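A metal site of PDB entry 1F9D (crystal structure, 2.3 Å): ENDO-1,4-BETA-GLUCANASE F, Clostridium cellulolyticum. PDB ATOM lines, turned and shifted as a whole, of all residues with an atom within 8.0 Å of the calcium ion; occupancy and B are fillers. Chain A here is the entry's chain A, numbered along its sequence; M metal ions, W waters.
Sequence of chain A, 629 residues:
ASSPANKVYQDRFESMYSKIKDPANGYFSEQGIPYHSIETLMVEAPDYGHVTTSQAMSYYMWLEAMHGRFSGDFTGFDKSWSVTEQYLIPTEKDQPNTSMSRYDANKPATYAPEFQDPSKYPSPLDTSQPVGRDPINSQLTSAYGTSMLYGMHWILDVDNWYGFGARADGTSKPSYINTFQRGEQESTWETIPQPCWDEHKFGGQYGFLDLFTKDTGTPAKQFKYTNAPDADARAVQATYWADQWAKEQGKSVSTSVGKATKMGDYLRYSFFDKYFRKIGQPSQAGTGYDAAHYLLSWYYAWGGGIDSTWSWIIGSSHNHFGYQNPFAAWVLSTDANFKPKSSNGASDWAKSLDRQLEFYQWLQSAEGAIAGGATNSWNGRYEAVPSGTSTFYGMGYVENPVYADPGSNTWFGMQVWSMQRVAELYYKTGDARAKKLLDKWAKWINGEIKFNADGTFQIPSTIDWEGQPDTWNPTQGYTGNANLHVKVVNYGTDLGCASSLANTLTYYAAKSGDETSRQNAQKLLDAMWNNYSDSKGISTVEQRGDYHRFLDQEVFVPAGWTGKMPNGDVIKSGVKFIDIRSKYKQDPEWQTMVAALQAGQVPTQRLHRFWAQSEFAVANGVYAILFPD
The side-chain carboxylate (OD1) of Asp 405 is in salt-bridge range of the guanidinium group (NH1) of Arg 549 (3.2 Å).
The side-chain carboxylate (OE2) of Glu 190 sits close to the guanidinium group (NH2) of Arg 549 (3.3 Å).
OE2 of Glu 190 lies close to OG of Ser 187 (2.8 Å).
OE2 of Glu 190 is bound to the calcium ion (2.3 Å).
The calcium ion is bound by O of Gln 185 (2.4 Å).
The calcium ion is bound by the side-chain amide oxygen (OE1) of Gln 185, at 2.4 Å.
The calcium ion is bound by OD2 of Asp 405 (2.4 Å).
The calcium ion is bound by water W2 (2.4 Å).
Water W1 binds the calcium ion (2.6 Å).
The calcium ion is bound by the side-chain carboxylate (OE1) of Glu 190, at 2.6 Å.
Within 4 Å of the calcium ion: Gln 185, Glu 190 and Asp 405.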
ATOM      1  N   GLN A 116     -20.661  14.886  -8.574  1.00  0.00           N
ATOM      2  CA  GLN A 116     -20.851  15.465  -9.899  1.00  0.00           C
ATOM      3  C   GLN A 116     -21.402  14.496 -10.947  1.00  0.00           C
ATOM      4  O   GLN A 116     -21.474  14.836 -12.129  1.00  0.00           O
ATOM      5  CB  GLN A 116     -19.545  16.081 -10.400  1.00  0.00           C
ATOM      6  CG  GLN A 116     -19.202  17.409  -9.726  1.00  0.00           C
ATOM      7  CD  GLN A 116     -19.055  17.301  -8.223  1.00  0.00           C
ATOM      8  OE1 GLN A 116     -18.144  16.618  -7.729  1.00  0.00           O
ATOM      9  NE2 GLN A 116     -19.933  17.968  -7.483  1.00  0.00           N
ATOM     10  N   ASP A 117     -21.797  13.302 -10.523  1.00  0.00           N
ATOM     11  CA  ASP A 117     -22.375  12.324 -11.435  1.00  0.00           C
ATOM     12  C   ASP A 117     -23.388  11.459 -10.699  1.00  0.00           C
ATOM     13  O   ASP A 117     -23.111  10.969  -9.613  1.00  0.00           O
ATOM     14  CB  ASP A 117     -21.302  11.422 -12.041  1.00  0.00           C
ATOM     15  CG  ASP A 117     -21.826  10.636 -13.228  1.00  0.00           C
ATOM     16  OD1 ASP A 117     -21.878  11.198 -14.336  1.00  0.00           O
ATOM     17  OD2 ASP A 117     -22.219   9.463 -13.039  1.00  0.00           O
ATOM     18  N   PRO A 118     -24.573  11.269 -11.285  1.00  0.00           N
ATOM     19  CA  PRO A 118     -25.597  10.458 -10.623  1.00  0.00           C
ATOM     20  C   PRO A 118     -25.163   9.032 -10.249  1.00  0.00           C
ATOM     21  O   PRO A 118     -25.708   8.460  -9.304  1.00  0.00           O
ATOM     22  CB  PRO A 118     -26.739  10.446 -11.640  1.00  0.00           C
ATOM     23  CG  PRO A 118     -26.589  11.761 -12.320  1.00  0.00           C
ATOM     24  CD  PRO A 118     -25.096  11.847 -12.528  1.00  0.00           C
ATOM     25  N   GLY A 183     -27.477  15.491  -7.546  1.00  0.00           N
ATOM     26  CA  GLY A 183     -26.481  16.414  -8.076  1.00  0.00           C
ATOM     27  C   GLY A 183     -26.667  17.182  -9.368  1.00  0.00           C
ATOM     28  O   GLY A 183     -27.683  17.052 -10.062  1.00  0.00           O
ATOM     29  N   GLU A 184     -25.642  17.963  -9.695  1.00  0.00           N
ATOM     30  CA  GLU A 184     -25.591  18.833 -10.870  1.00  0.00           C
ATOM     31  C   GLU A 184     -25.731  18.188 -12.243  1.00  0.00           C
ATOM     32  O   GLU A 184     -26.110  18.861 -13.195  1.00  0.00           O
ATOM     33  CB  GLU A 184     -24.305  19.657 -10.856  1.00  0.00           C
ATOM     34  CG  GLU A 184     -23.043  18.852 -11.208  1.00  0.00           C
ATOM     35  CD  GLU A 184     -21.796  19.717 -11.313  1.00  0.00           C
ATOM     36  OE1 GLU A 184     -21.605  20.605 -10.451  1.00  0.00           O
ATOM     37  OE2 GLU A 184     -20.984  19.493 -12.250  1.00  0.00           O
ATOM     38  N   GLN A 185     -25.397  16.915 -12.359  1.00  0.00           N
ATOM     39  CA  GLN A 185     -25.502  16.265 -13.659  1.00  0.00           C
ATOM     40  C   GLN A 185     -26.781  15.460 -13.790  1.00  0.00           C
ATOM     41  O   GLN A 185     -26.972  14.756 -14.778  1.00  0.00           O
ATOM     42  CB  GLN A 185     -24.293  15.366 -13.926  1.00  0.00           C
ATOM     43  CG  GLN A 185     -23.246  15.972 -14.867  1.00  0.00           C
ATOM     44  CD  GLN A 185     -23.803  16.275 -16.259  1.00  0.00           C
ATOM     45  OE1 GLN A 185     -24.679  15.560 -16.763  1.00  0.00           O
ATOM     46  NE2 GLN A 185     -23.273  17.319 -16.889  1.00  0.00           N
ATOM     47  N   GLU A 186     -27.665  15.541 -12.790  1.00  0.00           N
ATOM     48  CA  GLU A 186     -28.920  14.813 -12.889  1.00  0.00           C
ATOM     49  C   GLU A 186     -29.969  15.736 -13.470  1.00  0.00           C
ATOM     50  O   GLU A 186     -30.613  16.489 -12.738  1.00  0.00           O
ATOM     51  CB  GLU A 186     -29.383  14.310 -11.527  1.00  0.00           C
ATOM     52  CG  GLU A 186     -30.657  13.499 -11.634  1.00  0.00           C
ATOM     53  CD  GLU A 186     -31.250  13.137 -10.301  1.00  0.00           C
ATOM     54  OE1 GLU A 186     -31.429  14.051  -9.470  1.00  0.00           O
ATOM     55  OE2 GLU A 186     -31.550  11.946 -10.083  1.00  0.00           O
ATOM     56  N   SER A 187     -30.137  15.679 -14.788  1.00  0.00           N
ATOM     57  CA  SER A 187     -31.124  16.511 -15.460  1.00  0.00           C
ATOM     58  C   SER A 187     -32.517  15.992 -15.149  1.00  0.00           C
ATOM     59  O   SER A 187     -32.683  14.971 -14.474  1.00  0.00           O
ATOM     60  CB  SER A 187     -30.907  16.471 -16.970  1.00  0.00           C
ATOM     61  OG  SER A 187     -31.306  15.201 -17.498  1.00  0.00           O
ATOM     62  N   THR A 188     -33.524  16.696 -15.640  1.00  0.00           N
ATOM     63  CA  THR A 188     -34.902  16.316 -15.438  1.00  0.00           C
ATOM     64  C   THR A 188     -35.168  14.961 -16.100  1.00  0.00           C
ATOM     65  O   THR A 188     -36.110  14.254 -15.736  1.00  0.00           O
ATOM     66  CB  THR A 188     -35.862  17.380 -16.031  1.00  0.00           C
ATOM     67  OG1 THR A 188     -37.218  16.976 -15.845  1.00  0.00           O
ATOM     68  CG2 THR A 188     -35.595  17.558 -17.513  1.00  0.00           C
ATOM     69  N   TRP A 189     -34.310  14.588 -17.048  1.00  0.00           N
ATOM     70  CA  TRP A 189     -34.442  13.310 -17.755  1.00  0.00           C
ATOM     71  C   TRP A 189     -33.760  12.134 -17.054  1.00  0.00           C
ATOM     72  O   TRP A 189     -33.945  10.987 -17.460  1.00  0.00           O
ATOM     73  CB  TRP A 189     -33.850  13.405 -19.168  1.00  0.00           C
ATOM     74  CG  TRP A 189     -34.409  14.494 -20.022  1.00  0.00           C
ATOM     75  CD1 TRP A 189     -33.923  15.760 -20.151  1.00  0.00           C
ATOM     76  CD2 TRP A 189     -35.543  14.404 -20.880  1.00  0.00           C
ATOM     77  NE1 TRP A 189     -34.692  16.473 -21.029  1.00  0.00           N
ATOM     78  CE2 TRP A 189     -35.695  15.672 -21.496  1.00  0.00           C
ATOM     79  CE3 TRP A 189     -36.456  13.382 -21.185  1.00  0.00           C
ATOM     80  CZ2 TRP A 189     -36.722  15.938 -22.396  1.00  0.00           C
ATOM     81  CZ3 TRP A 189     -37.475  13.642 -22.084  1.00  0.00           C
ATOM     82  CH2 TRP A 189     -37.596  14.920 -22.686  1.00  0.00           C
ATOM     83  N   GLU A 190     -32.979  12.409 -16.011  1.00  0.00           N
ATOM     84  CA  GLU A 190     -32.231  11.359 -15.334  1.00  0.00           C
ATOM     85  C   GLU A 190     -32.661  11.022 -13.911  1.00  0.00           C
ATOM     86  O   GLU A 190     -31.934  10.343 -13.171  1.00  0.00           O
ATOM     87  CB  GLU A 190     -30.747  11.721 -15.347  1.00  0.00           C
ATOM     88  CG  GLU A 190     -30.211  11.934 -16.744  1.00  0.00           C
ATOM     89  CD  GLU A 190     -28.884  12.666 -16.774  1.00  0.00           C
ATOM     90  OE1 GLU A 190     -27.836  12.035 -16.544  1.00  0.00           O
ATOM     91  OE2 GLU A 190     -28.912  13.893 -17.022  1.00  0.00           O
ATOM     92  N   ALA A 404     -25.776  21.573 -14.246  1.00  0.00           N
ATOM     93  CA  ALA A 404     -24.921  21.678 -15.412  1.00  0.00           C
ATOM     94  C   ALA A 404     -25.537  21.031 -16.653  1.00  0.00           C
ATOM     95  O   ALA A 404     -24.998  21.157 -17.748  1.00  0.00           O
ATOM     96  CB  ALA A 404     -23.550  21.031 -15.116  1.00  0.00           C
ATOM     97  N   ASP A 405     -26.666  20.349 -16.483  1.00  0.00           N
ATOM     98  CA  ASP A 405     -27.332  19.644 -17.587  1.00  0.00           C
ATOM     99  C   ASP A 405     -28.804  20.051 -17.757  1.00  0.00           C
ATOM    100  O   ASP A 405     -29.701  19.345 -17.291  1.00  0.00           O
ATOM    101  CB  ASP A 405     -27.211  18.127 -17.346  1.00  0.00           C
ATOM    102  CG  ASP A 405     -27.738  17.274 -18.507  1.00  0.00           C
ATOM    103  OD1 ASP A 405     -28.111  17.826 -19.563  1.00  0.00           O
ATOM    104  OD2 ASP A 405     -27.766  16.035 -18.346  1.00  0.00           O
ATOM    105  N   PRO A 406     -29.074  21.195 -18.397  1.00  0.00           N
ATOM    106  CA  PRO A 406     -28.121  22.149 -18.987  1.00  0.00           C
ATOM    107  C   PRO A 406     -27.696  23.169 -17.923  1.00  0.00           C
ATOM    108  O   PRO A 406     -28.219  23.160 -16.811  1.00  0.00           O
ATOM    109  CB  PRO A 406     -28.934  22.779 -20.109  1.00  0.00           C
ATOM    110  CG  PRO A 406     -30.296  22.886 -19.484  1.00  0.00           C
ATOM    111  CD  PRO A 406     -30.461  21.533 -18.797  1.00  0.00           C
ATOM    112  N   ARG A 549     -34.396  12.361 -25.692  1.00  0.00           N
ATOM    113  CA  ARG A 549     -34.035  11.732 -24.421  1.00  0.00           C
ATOM    114  C   ARG A 549     -35.167  10.873 -23.836  1.00  0.00           C
ATOM    115  O   ARG A 549     -34.925  10.061 -22.943  1.00  0.00           O
ATOM    116  CB  ARG A 549     -33.564  12.801 -23.435  1.00  0.00           C
ATOM    117  CG  ARG A 549     -32.417  13.615 -24.005  1.00  0.00           C
ATOM    118  CD  ARG A 549     -31.900  14.702 -23.074  1.00  0.00           C
ATOM    119  NE  ARG A 549     -31.104  14.164 -21.986  1.00  0.00           N
ATOM    120  CZ  ARG A 549     -30.322  14.913 -21.193  1.00  0.00           C
ATOM    121  NH1 ARG A 549     -30.250  16.224 -21.388  1.00  0.00           N
ATOM    122  NH2 ARG A 549     -29.622  14.351 -20.225  1.00  0.00           N
ATOM    123  N   GLN A 553     -32.344   8.314 -23.192  1.00  0.00           N
ATOM    124  CA  GLN A 553     -31.673   8.656 -21.936  1.00  0.00           C
ATOM    125  C   GLN A 553     -31.728   7.507 -20.954  1.00  0.00           C
ATOM    126  O   GLN A 553     -32.808   7.100 -20.496  1.00  0.00           O
ATOM    127  CB  GLN A 553     -32.302   9.891 -21.274  1.00  0.00           C
ATOM    128  CG  GLN A 553     -31.629  10.250 -19.949  1.00  0.00           C
ATOM    129  CD  GLN A 553     -30.196  10.731 -20.132  1.00  0.00           C
ATOM    130  OE1 GLN A 553     -29.950  11.787 -20.690  1.00  0.00           O
ATOM    131  NE2 GLN A 553     -29.239   9.934 -19.664  1.00  0.00           N
ATOM    132  N   GLU A 554     -30.574   6.962 -20.628  1.00  0.00           N
ATOM    133  CA  GLU A 554     -30.511   5.872 -19.672  1.00  0.00           C
ATOM    134  C   GLU A 554     -30.583   6.497 -18.288  1.00  0.00           C
ATOM    135  O   GLU A 554     -30.025   7.565 -18.035  1.00  0.00           O
ATOM    136  CB  GLU A 554     -29.193   5.099 -19.839  1.00  0.00           C
ATOM    137  CG  GLU A 554     -29.113   3.808 -19.022  1.00  0.00           C
ATOM    138  CD  GLU A 554     -27.761   3.114 -19.138  1.00  0.00           C
ATOM    139  OE1 GLU A 554     -27.369   2.788 -20.287  1.00  0.00           O
ATOM    140  OE2 GLU A 554     -27.102   2.914 -18.101  1.00  0.00           O
HETATM  141 CA    CA M   1     -26.662  14.305 -17.078  1.00  0.00          CA
HETATM  142  O   HOH W   1     -26.442  13.164 -19.359  1.00  0.00           O
HETATM  143  O   HOH W   2     -24.982  12.681 -16.352  1.00  0.00           O
